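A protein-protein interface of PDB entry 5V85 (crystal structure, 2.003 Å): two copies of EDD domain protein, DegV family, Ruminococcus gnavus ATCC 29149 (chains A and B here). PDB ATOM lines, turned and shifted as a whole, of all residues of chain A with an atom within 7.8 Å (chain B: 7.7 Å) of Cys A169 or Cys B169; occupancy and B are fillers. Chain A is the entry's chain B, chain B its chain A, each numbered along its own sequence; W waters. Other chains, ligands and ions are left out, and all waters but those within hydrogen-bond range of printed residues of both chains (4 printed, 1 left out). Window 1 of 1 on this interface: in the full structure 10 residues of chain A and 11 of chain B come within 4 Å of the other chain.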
ATOM      1  N   PHE A 134      -2.288 -36.941  14.219  1.00  0.00           N
ATOM      2  CA  PHE A 134      -2.038 -35.515  14.390  1.00  0.00           C
ATOM      3  C   PHE A 134      -0.703 -35.153  13.749  1.00  0.00           C
ATOM      4  O   PHE A 134       0.350 -35.626  14.194  1.00  0.00           O
ATOM      5  CB  PHE A 134      -2.012 -35.130  15.870  1.00  0.00           C
ATOM      6  CG  PHE A 134      -3.339 -35.246  16.566  1.00  0.00           C
ATOM      7  CD1 PHE A 134      -4.333 -34.301  16.358  1.00  0.00           C
ATOM      8  CD2 PHE A 134      -3.579 -36.286  17.452  1.00  0.00           C
ATOM      9  CE1 PHE A 134      -5.549 -34.402  17.008  1.00  0.00           C
ATOM     10  CE2 PHE A 134      -4.792 -36.394  18.106  1.00  0.00           C
ATOM     11  CZ  PHE A 134      -5.780 -35.450  17.886  1.00  0.00           C
ATOM     12  N   LYS A 149      -1.644 -33.199  25.776  1.00  0.00           N
ATOM     13  CA  LYS A 149      -2.948 -32.571  25.589  1.00  0.00           C
ATOM     14  C   LYS A 149      -4.018 -33.606  25.263  1.00  0.00           C
ATOM     15  O   LYS A 149      -5.158 -33.495  25.732  1.00  0.00           O
ATOM     16  CB  LYS A 149      -2.872 -31.504  24.496  1.00  0.00           C
ATOM     17  CG  LYS A 149      -4.209 -30.831  24.208  1.00  0.00           C
ATOM     18  CD  LYS A 149      -4.217 -29.366  24.628  1.00  0.00           C
ATOM     19  CE  LYS A 149      -3.725 -29.170  26.049  1.00  0.00           C
ATOM     20  NZ  LYS A 149      -4.396 -28.021  26.718  1.00  0.00           N
ATOM     21  N   VAL A 163     -11.982 -34.791  21.361  1.00  0.00           N
ATOM     22  CA  VAL A 163     -10.539 -34.770  21.596  1.00  0.00           C
ATOM     23  C   VAL A 163      -9.810 -34.295  20.347  1.00  0.00           C
ATOM     24  O   VAL A 163      -8.923 -33.435  20.411  1.00  0.00           O
ATOM     25  CB  VAL A 163     -10.038 -36.159  22.035  1.00  0.00           C
ATOM     26  CG1 VAL A 163      -8.514 -36.163  22.112  1.00  0.00           C
ATOM     27  CG2 VAL A 163     -10.637 -36.556  23.370  1.00  0.00           C
ATOM     28  N   VAL A 164     -10.180 -34.847  19.189  1.00  0.00           N
ATOM     29  CA  VAL A 164      -9.497 -34.509  17.943  1.00  0.00           C
ATOM     30  C   VAL A 164      -9.591 -33.012  17.673  1.00  0.00           C
ATOM     31  O   VAL A 164      -8.593 -32.357  17.349  1.00  0.00           O
ATOM     32  CB  VAL A 164     -10.076 -35.328  16.774  1.00  0.00           C
ATOM     33  CG1 VAL A 164      -9.561 -34.789  15.448  1.00  0.00           C
ATOM     34  CG2 VAL A 164      -9.726 -36.805  16.928  1.00  0.00           C
ATOM     35  N   GLU A 165     -10.796 -32.449  17.809  1.00  0.00           N
ATOM     36  CA  GLU A 165     -10.984 -31.032  17.515  1.00  0.00           C
ATOM     37  C   GLU A 165     -10.225 -30.156  18.504  1.00  0.00           C
ATOM     38  O   GLU A 165      -9.620 -29.150  18.114  1.00  0.00           O
ATOM     39  CB  GLU A 165     -12.476 -30.687  17.523  1.00  0.00           C
ATOM     40  CG  GLU A 165     -12.851 -29.562  16.569  1.00  0.00           C
ATOM     41  CD  GLU A 165     -14.309 -29.139  16.683  1.00  0.00           C
ATOM     42  OE1 GLU A 165     -14.814 -28.507  15.733  1.00  0.00           O
ATOM     43  OE2 GLU A 165     -14.948 -29.431  17.718  1.00  0.00           O
ATOM     44  N   SER A 166     -10.235 -30.527  19.786  1.00  0.00           N
ATOM     45  CA  SER A 166      -9.551 -29.718  20.790  1.00  0.00           C
ATOM     46  C   SER A 166      -8.040 -29.768  20.606  1.00  0.00           C
ATOM     47  O   SER A 166      -7.354 -28.754  20.779  1.00  0.00           O
ATOM     48  CB  SER A 166      -9.934 -30.187  22.192  1.00  0.00           C
ATOM     49  OG  SER A 166     -11.127 -29.564  22.626  1.00  0.00           O
ATOM     50  N   VAL A 167      -7.501 -30.936  20.254  1.00  0.00           N
ATOM     51  CA  VAL A 167      -6.057 -31.049  20.088  1.00  0.00           C
ATOM     52  C   VAL A 167      -5.601 -30.309  18.833  1.00  0.00           C
ATOM     53  O   VAL A 167      -4.535 -29.681  18.823  1.00  0.00           O
ATOM     54  CB  VAL A 167      -5.633 -32.530  20.077  1.00  0.00           C
ATOM     55  CG1 VAL A 167      -4.155 -32.662  19.735  1.00  0.00           C
ATOM     56  CG2 VAL A 167      -5.909 -33.162  21.439  1.00  0.00           C
ATOM     57  N   GLU A 168      -6.396 -30.359  17.760  1.00  0.00           N
ATOM     58  CA  GLU A 168      -6.022 -29.616  16.561  1.00  0.00           C
ATOM     59  C   GLU A 168      -6.036 -28.114  16.814  1.00  0.00           C
ATOM     60  O   GLU A 168      -5.215 -27.383  16.247  1.00  0.00           O
ATOM     61  CB  GLU A 168      -6.945 -29.977  15.396  1.00  0.00           C
ATOM     62  CG  GLU A 168      -6.745 -31.393  14.856  1.00  0.00           C
ATOM     63  CD  GLU A 168      -5.492 -31.542  14.000  1.00  0.00           C
ATOM     64  OE1 GLU A 168      -4.832 -30.523  13.703  1.00  0.00           O
ATOM     65  OE2 GLU A 168      -5.169 -32.689  13.621  1.00  0.00           O
ATOM     66  N   CYS A 169      -6.949 -27.637  17.666  1.00  0.00           N
ATOM     67  CA  CYS A 169      -6.929 -26.234  18.065  1.00  0.00           C
ATOM     68  C   CYS A 169      -5.640 -25.898  18.802  1.00  0.00           C
ATOM     69  O   CYS A 169      -5.017 -24.863  18.542  1.00  0.00           O
ATOM     70  CB  CYS A 169      -8.127 -25.928  18.962  1.00  0.00           C
ATOM     71  SG  CYS A 169      -9.695 -25.620  18.128  1.00  0.00           S
ATOM     72  N   TYR A 170      -5.232 -26.762  19.735  1.00  0.00           N
ATOM     73  CA  TYR A 170      -3.993 -26.526  20.468  1.00  0.00           C
ATOM     74  C   TYR A 170      -2.796 -26.487  19.527  1.00  0.00           C
ATOM     75  O   TYR A 170      -1.910 -25.637  19.677  1.00  0.00           O
ATOM     76  CB  TYR A 170      -3.800 -27.603  21.539  1.00  0.00           C
ATOM     77  CG  TYR A 170      -2.414 -27.598  22.145  1.00  0.00           C
ATOM     78  CD1 TYR A 170      -2.007 -26.567  22.985  1.00  0.00           C
ATOM     79  CD2 TYR A 170      -1.505 -28.609  21.863  1.00  0.00           C
ATOM     80  CE1 TYR A 170      -0.734 -26.546  23.534  1.00  0.00           C
ATOM     81  CE2 TYR A 170      -0.227 -28.598  22.409  1.00  0.00           C
ATOM     82  CZ  TYR A 170       0.152 -27.563  23.243  1.00  0.00           C
ATOM     83  OH  TYR A 170       1.418 -27.542  23.787  1.00  0.00           O
ATOM     84  N   ILE A 171      -2.755 -27.400  18.550  1.00  0.00           N
ATOM     85  CA  ILE A 171      -1.645 -27.438  17.599  1.00  0.00           C
ATOM     86  C   ILE A 171      -1.503 -26.098  16.885  1.00  0.00           C
ATOM     87  O   ILE A 171      -0.386 -25.606  16.679  1.00  0.00           O
ATOM     88  CB  ILE A 171      -1.837 -28.601  16.604  1.00  0.00           C
ATOM     89  CG1 ILE A 171      -1.672 -29.943  17.324  1.00  0.00           C
ATOM     90  CG2 ILE A 171      -0.861 -28.483  15.432  1.00  0.00           C
ATOM     91  CD1 ILE A 171      -1.957 -31.143  16.459  1.00  0.00           C
ATOM     92  N   GLU A 172      -2.626 -25.482  16.505  1.00  0.00           N
ATOM     93  CA  GLU A 172      -2.566 -24.172  15.862  1.00  0.00           C
ATOM     94  C   GLU A 172      -2.030 -23.102  16.808  1.00  0.00           C
ATOM     95  O   GLU A 172      -1.386 -22.147  16.359  1.00  0.00           O
ATOM     96  CB  GLU A 172      -3.948 -23.773  15.340  1.00  0.00           C
ATOM     97  CG  GLU A 172      -3.947 -22.519  14.474  1.00  0.00           C
ATOM     98  CD  GLU A 172      -5.252 -21.742  14.552  1.00  0.00           C
ATOM     99  OE1 GLU A 172      -5.552 -21.172  15.625  1.00  0.00           O
ATOM    100  OE2 GLU A 172      -5.976 -21.700  13.534  1.00  0.00           O
ATOM    101  N   GLU A 173      -2.287 -23.243  18.112  1.00  0.00           N
ATOM    102  CA  GLU A 173      -1.731 -22.321  19.098  1.00  0.00           C
ATOM    103  C   GLU A 173      -0.249 -22.548  19.328  1.00  0.00           C
ATOM    104  O   GLU A 173       0.458 -21.633  19.768  1.00  0.00           O
ATOM    105  CB  GLU A 173      -2.419 -22.510  20.440  1.00  0.00           C
ATOM    106  CG  GLU A 173      -3.758 -21.909  20.594  1.00  0.00           C
ATOM    107  CD  GLU A 173      -4.152 -21.893  22.047  1.00  0.00           C
ATOM    108  OE1 GLU A 173      -4.103 -20.809  22.659  1.00  0.00           O
ATOM    109  OE2 GLU A 173      -4.474 -22.975  22.582  1.00  0.00           O
ATOM    110  N   GLN A 174       0.220 -23.770  19.103  1.00  0.00           N
ATOM    111  CA  GLN A 174       1.531 -24.188  19.569  1.00  0.00           C
ATOM    112  C   GLN A 174       2.621 -23.638  18.661  1.00  0.00           C
ATOM    113  O   GLN A 174       2.532 -23.746  17.434  1.00  0.00           O
ATOM    114  CB  GLN A 174       1.595 -25.712  19.625  1.00  0.00           C
ATOM    115  CG  GLN A 174       2.759 -26.271  20.421  1.00  0.00           C
ATOM    116  CD  GLN A 174       2.964 -27.754  20.173  1.00  0.00           C
ATOM    117  OE1 GLN A 174       3.061 -28.195  19.028  1.00  0.00           O
ATOM    118  NE2 GLN A 174       3.023 -28.533  21.249  1.00  0.00           N
ATOM    119  N   LYS A 247      -0.963 -23.349  30.349  1.00  0.00           N
ATOM    120  CA  LYS A 247      -0.232 -24.211  29.437  1.00  0.00           C
ATOM    121  C   LYS A 247       1.027 -24.763  30.091  1.00  0.00           C
ATOM    122  O   LYS A 247       1.563 -24.205  31.053  1.00  0.00           O
ATOM    123  CB  LYS A 247       0.125 -23.458  28.150  1.00  0.00           C
ATOM    124  CG  LYS A 247      -1.066 -23.270  27.216  1.00  0.00           C
ATOM    125  CD  LYS A 247      -0.745 -22.325  26.074  1.00  0.00           C
ATOM    126  CE  LYS A 247      -1.931 -22.185  25.127  1.00  0.00           C
ATOM    127  NZ  LYS A 247      -1.671 -21.137  24.105  1.00  0.00           N
ATOM    128  N   PHE B 134      -9.689 -10.259  17.012  1.00  0.00           N
ATOM    129  CA  PHE B 134      -9.887 -11.562  16.386  1.00  0.00           C
ATOM    130  C   PHE B 134     -10.036 -11.386  14.878  1.00  0.00           C
ATOM    131  O   PHE B 134     -10.977 -10.732  14.415  1.00  0.00           O
ATOM    132  CB  PHE B 134     -11.127 -12.260  16.948  1.00  0.00           C
ATOM    133  CG  PHE B 134     -11.033 -12.604  18.408  1.00  0.00           C
ATOM    134  CD1 PHE B 134     -10.285 -13.692  18.832  1.00  0.00           C
ATOM    135  CD2 PHE B 134     -11.704 -11.847  19.353  1.00  0.00           C
ATOM    136  CE1 PHE B 134     -10.200 -14.012  20.179  1.00  0.00           C
ATOM    137  CE2 PHE B 134     -11.627 -12.161  20.698  1.00  0.00           C
ATOM    138  CZ  PHE B 134     -10.873 -13.244  21.112  1.00  0.00           C
ATOM    139  N   LYS B 149     -19.586 -16.240  20.724  1.00  0.00           N
ATOM    140  CA  LYS B 149     -18.668 -17.122  21.437  1.00  0.00           C
ATOM    141  C   LYS B 149     -17.914 -16.369  22.527  1.00  0.00           C
ATOM    142  O   LYS B 149     -17.686 -16.905  23.618  1.00  0.00           O
ATOM    143  CB  LYS B 149     -17.693 -17.768  20.451  1.00  0.00           C
ATOM    144  CG  LYS B 149     -16.665 -18.707  21.084  1.00  0.00           C
ATOM    145  CD  LYS B 149     -17.343 -19.826  21.863  1.00  0.00           C
ATOM    146  CE  LYS B 149     -18.063 -20.789  20.932  1.00  0.00           C
ATOM    147  NZ  LYS B 149     -18.473 -22.039  21.633  1.00  0.00           N
ATOM    148  N   VAL B 163     -10.459 -16.495  27.336  1.00  0.00           N
ATOM    149  CA  VAL B 163     -11.404 -16.139  26.278  1.00  0.00           C
ATOM    150  C   VAL B 163     -10.703 -16.114  24.931  1.00  0.00           C
ATOM    151  O   VAL B 163     -11.207 -16.661  23.942  1.00  0.00           O
ATOM    152  CB  VAL B 163     -12.104 -14.802  26.585  1.00  0.00           C
ATOM    153  CG1 VAL B 163     -13.053 -14.444  25.444  1.00  0.00           C
ATOM    154  CG2 VAL B 163     -12.872 -14.883  27.897  1.00  0.00           C
ATOM    155  N   VAL B 164      -9.517 -15.504  24.877  1.00  0.00           N
ATOM    156  CA  VAL B 164      -8.790 -15.404  23.615  1.00  0.00           C
ATOM    157  C   VAL B 164      -8.511 -16.792  23.051  1.00  0.00           C
ATOM    158  O   VAL B 164      -8.762 -17.063  21.871  1.00  0.00           O
ATOM    159  CB  VAL B 164      -7.494 -14.597  23.809  1.00  0.00           C
ATOM    160  CG1 VAL B 164      -6.615 -14.704  22.577  1.00  0.00           C
ATOM    161  CG2 VAL B 164      -7.818 -13.139  24.110  1.00  0.00           C
ATOM    162  N   GLU B 165      -8.015 -17.702  23.897  1.00  0.00           N
ATOM    163  CA  GLU B 165      -7.662 -19.041  23.430  1.00  0.00           C
ATOM    164  C   GLU B 165      -8.886 -19.801  22.927  1.00  0.00           C
ATOM    165  O   GLU B 165      -8.845 -20.433  21.865  1.00  0.00           O
ATOM    166  CB  GLU B 165      -6.970 -19.820  24.551  1.00  0.00           C
ATOM    167  CG  GLU B 165      -6.779 -21.300  24.251  1.00  0.00           C
ATOM    168  CD  GLU B 165      -5.952 -22.015  25.311  1.00  0.00           C
ATOM    169  OE1 GLU B 165      -5.799 -21.471  26.424  1.00  0.00           O
ATOM    170  OE2 GLU B 165      -5.452 -23.123  25.032  1.00  0.00           O
ATOM    171  N   SER B 166      -9.989 -19.758  23.682  1.00  0.00           N
ATOM    172  CA  SER B 166     -11.175 -20.516  23.286  1.00  0.00           C
ATOM    173  C   SER B 166     -11.811 -19.948  22.023  1.00  0.00           C
ATOM    174  O   SER B 166     -12.333 -20.701  21.191  1.00  0.00           O
ATOM    175  CB  SER B 166     -12.198 -20.537  24.418  1.00  0.00           C
ATOM    176  OG  SER B 166     -11.732 -21.294  25.519  1.00  0.00           O
ATOM    177  N   VAL B 167     -11.798 -18.623  21.869  1.00  0.00           N
ATOM    178  CA  VAL B 167     -12.404 -18.021  20.686  1.00  0.00           C
ATOM    179  C   VAL B 167     -11.531 -18.262  19.461  1.00  0.00           C
ATOM    180  O   VAL B 167     -12.039 -18.493  18.358  1.00  0.00           O
ATOM    181  CB  VAL B 167     -12.671 -16.524  20.922  1.00  0.00           C
ATOM    182  CG1 VAL B 167     -13.124 -15.854  19.635  1.00  0.00           C
ATOM    183  CG2 VAL B 167     -13.726 -16.350  22.004  1.00  0.00           C
ATOM    184  N   GLU B 168     -10.207 -18.225  19.626  1.00  0.00           N
ATOM    185  CA  GLU B 168      -9.344 -18.548  18.494  1.00  0.00           C
ATOM    186  C   GLU B 168      -9.490 -20.009  18.082  1.00  0.00           C
ATOM    187  O   GLU B 168      -9.340 -20.331  16.898  1.00  0.00           O
ATOM    188  CB  GLU B 168      -7.885 -18.218  18.817  1.00  0.00           C
ATOM    189  CG  GLU B 168      -7.594 -16.722  18.938  1.00  0.00           C
ATOM    190  CD  GLU B 168      -7.532 -16.004  17.594  1.00  0.00           C
ATOM    191  OE1 GLU B 168      -7.645 -16.672  16.543  1.00  0.00           O
ATOM    192  OE2 GLU B 168      -7.369 -14.763  17.593  1.00  0.00           O
ATOM    193  N   CYS B 169      -9.789 -20.903  19.031  1.00  0.00           N
ATOM    194  CA  CYS B 169     -10.074 -22.289  18.670  1.00  0.00           C
ATOM    195  C   CYS B 169     -11.382 -22.390  17.895  1.00  0.00           C
ATOM    196  O   CYS B 169     -11.464 -23.104  16.890  1.00  0.00           O
ATOM    197  CB  CYS B 169     -10.126 -23.170  19.920  1.00  0.00           C
ATOM    198  SG  CYS B 169     -10.830 -24.831  19.630  1.00  0.00           S
ATOM    199  N   TYR B 170     -12.423 -21.685  18.352  1.00  0.00           N
ATOM    200  CA  TYR B 170     -13.689 -21.698  17.627  1.00  0.00           C
ATOM    201  C   TYR B 170     -13.520 -21.164  16.210  1.00  0.00           C
ATOM    202  O   TYR B 170     -14.124 -21.689  15.266  1.00  0.00           O
ATOM    203  CB  TYR B 170     -14.752 -20.881  18.362  1.00  0.00           C
ATOM    204  CG  TYR B 170     -15.997 -20.696  17.513  1.00  0.00           C
ATOM    205  CD1 TYR B 170     -16.776 -21.788  17.150  1.00  0.00           C
ATOM    206  CD2 TYR B 170     -16.370 -19.441  17.042  1.00  0.00           C
ATOM    207  CE1 TYR B 170     -17.901 -21.639  16.361  1.00  0.00           C
ATOM    208  CE2 TYR B 170     -17.503 -19.280  16.246  1.00  0.00           C
ATOM    209  CZ  TYR B 170     -18.261 -20.385  15.911  1.00  0.00           C
ATOM    210  OH  TYR B 170     -19.385 -20.251  15.123  1.00  0.00           O
ATOM    211  N   ILE B 171     -12.711 -20.115  16.044  1.00  0.00           N
ATOM    212  CA  ILE B 171     -12.451 -19.578  14.709  1.00  0.00           C
ATOM    213  C   ILE B 171     -11.829 -20.649  13.821  1.00  0.00           C
ATOM    214  O   ILE B 171     -12.174 -20.774  12.639  1.00  0.00           O
ATOM    215  CB  ILE B 171     -11.562 -18.323  14.805  1.00  0.00           C
ATOM    216  CG1 ILE B 171     -12.340 -17.168  15.448  1.00  0.00           C
ATOM    217  CG2 ILE B 171     -11.034 -17.919  13.433  1.00  0.00           C
ATOM    218  CD1 ILE B 171     -11.516 -15.909  15.638  1.00  0.00           C
ATOM    219  N   GLU B 172     -10.922 -21.451  14.383  1.00  0.00           N
ATOM    220  CA  GLU B 172     -10.296 -22.530  13.624  1.00  0.00           C
ATOM    221  C   GLU B 172     -11.299 -23.617  13.249  1.00  0.00           C
ATOM    222  O   GLU B 172     -11.182 -24.224  12.179  1.00  0.00           O
ATOM    223  CB  GLU B 172      -9.139 -23.126  14.429  1.00  0.00           C
ATOM    224  CG  GLU B 172      -8.326 -24.173  13.681  1.00  0.00           C
ATOM    225  CD  GLU B 172      -8.682 -25.593  14.083  1.00  0.00           C
ATOM    226  OE1 GLU B 172      -9.536 -25.764  14.977  1.00  0.00           O
ATOM    227  OE2 GLU B 172      -8.110 -26.538  13.501  1.00  0.00           O
ATOM    228  N   GLU B 173     -12.284 -23.875  14.110  1.00  0.00           N
ATOM    229  CA  GLU B 173     -13.317 -24.858  13.801  1.00  0.00           C
ATOM    230  C   GLU B 173     -14.376 -24.317  12.850  1.00  0.00           C
ATOM    231  O   GLU B 173     -15.062 -25.106  12.190  1.00  0.00           O
ATOM    232  CB  GLU B 173     -13.992 -25.336  15.090  1.00  0.00           C
ATOM    233  CG  GLU B 173     -13.020 -25.849  16.148  1.00  0.00           C
ATOM    234  CD  GLU B 173     -13.653 -25.963  17.526  1.00  0.00           C
ATOM    235  OE1 GLU B 173     -14.645 -25.254  17.796  1.00  0.00           O
ATOM    236  OE2 GLU B 173     -13.157 -26.767  18.342  1.00  0.00           O
ATOM    237  N   GLN B 174     -14.512 -22.997  12.759  1.00  0.00           N
ATOM    238  CA  GLN B 174     -15.604 -22.374  12.022  1.00  0.00           C
ATOM    239  C   GLN B 174     -15.347 -22.393  10.518  1.00  0.00           C
ATOM    240  O   GLN B 174     -14.244 -22.078  10.061  1.00  0.00           O
ATOM    241  CB  GLN B 174     -15.786 -20.937  12.509  1.00  0.00           C
ATOM    242  CG  GLN B 174     -17.033 -20.238  12.004  1.00  0.00           C
ATOM    243  CD  GLN B 174     -17.023 -18.751  12.318  1.00  0.00           C
ATOM    244  OE1 GLN B 174     -16.157 -18.013  11.851  1.00  0.00           O
ATOM    245  NE2 GLN B 174     -17.987 -18.307  13.121  1.00  0.00           N
ATOM    246  N   LYS B 247     -22.545 -26.569  18.568  1.00  0.00           N
ATOM    247  CA  LYS B 247     -22.347 -25.364  17.780  1.00  0.00           C
ATOM    248  C   LYS B 247     -23.674 -24.747  17.361  1.00  0.00           C
ATOM    249  O   LYS B 247     -24.694 -25.432  17.237  1.00  0.00           O
ATOM    250  CB  LYS B 247     -21.490 -25.669  16.545  1.00  0.00           C
ATOM    251  CG  LYS B 247     -20.270 -26.514  16.879  1.00  0.00           C
ATOM    252  CD  LYS B 247     -19.299 -26.617  15.726  1.00  0.00           C
ATOM    253  CE  LYS B 247     -17.977 -27.212  16.192  1.00  0.00           C
ATOM    254  NZ  LYS B 247     -17.026 -27.380  15.062  1.00  0.00           N
HETATM  255  O   HOH W   1      -7.660 -18.984  15.155  1.00  0.00           O
HETATM  256  O   HOH W   2     -10.149 -28.107  15.281  1.00  0.00           O
HETATM  257  O   HOH W   3      -6.734 -21.661  20.697  1.00  0.00           O
HETATM  258  O   HOH W   4     -14.228 -28.075  12.512  1.00  0.00           O
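OE2 of Glu B165 lies close to OE2 of Glu A173 (2.6 Å).
SG of Cys A169 forms a disulfide with SG of Cys B169 (2.0 Å).
The side-chain amino group (NZ) of Lys B247 lies within salt-bridge range of the side-chain carboxylate (OE1) of Glu A165 (2.6 Å).
OE2 of Glu A165 lies close to OE2 of Glu B173, 3.3 Å away.
OE1 of Glu B172 sits close to SG of Cys A169 (3.2 Å).
SG of Cys A169 sits close to OE2 of Glu B173 (3.7 Å).
The side-chain carboxylate of Glu A173 lies within salt-bridge range of the side-chain amino group of Lys A247 (2.8 Å).
Glu B172 touches Glu A172.
Lys A247 touches Glu B165 (CE to OE2, 3.6 Å).
Cys A169 touches just these residues of chain B: Cys B169, Glu B172 and Glu B173.
Cys B169 touches just one residue of chain A: Cys A169 (2.0 Å).
Printed residues of chain B within 4 Å of Glu A165: Glu B173 and Lys B247.
Printed residues of chain A within 4 Å of Lys B247: Glu A165 (2.6 Å).
Of the printed residues of chain B, Lys A247 touches Glu B165.
Val A167 touches none of the printed residues of chain B.
Val A164 touches none of the printed residues of chain B.
The nearest residue of chain B that does not touch Cys A169 is Tyr B170 (4.8 Å).
Printed residues of chain B that touch a printed residue of chain A: Glu B165, Cys B169, Glu B172, Glu B173 and Lys B247.
Glu A165 touches Glu B173, and with the chains exchanged Glu A173 touches Glu B165.
Glu A165 touches Lys B247, and with the chains exchanged Lys A247 touches Glu B165.
Cys B169 touches its own counterpart, Cys A169.
Cys A169 touches Glu B173, but with the chains exchanged Glu A173 does not touch Cys B169 (6.3 Å).
Positions printed for both chains: 134, 149, 163, 164, 165, 166, 167, 168, 169, 170, 171, 172, 173, 174 and 247.
Of the 8 pairs that touch across the chains among the printed residues, 6 have their exchanged pair printed and touching as well.
Water W2 bridges the side-chain carboxylate (OE1) of Glu B172 (2.4 Å) and the backbone carbonyl oxygen (O) of Glu A165 (3.1 Å).
Water W1 lies within hydrogen-bond range of the side-chain carboxylate (OE1) of Glu B168 and the side-chain carboxylate (OE1) of Glu A172.
Water W3 bridges O of Glu B165 (2.7 Å) and OE2 of Glu A173 (3.2 Å).
Water W4 lies within hydrogen-bond range of O of Glu B173 (3.1 Å) and OE1 of Glu A165 (3.3 Å).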
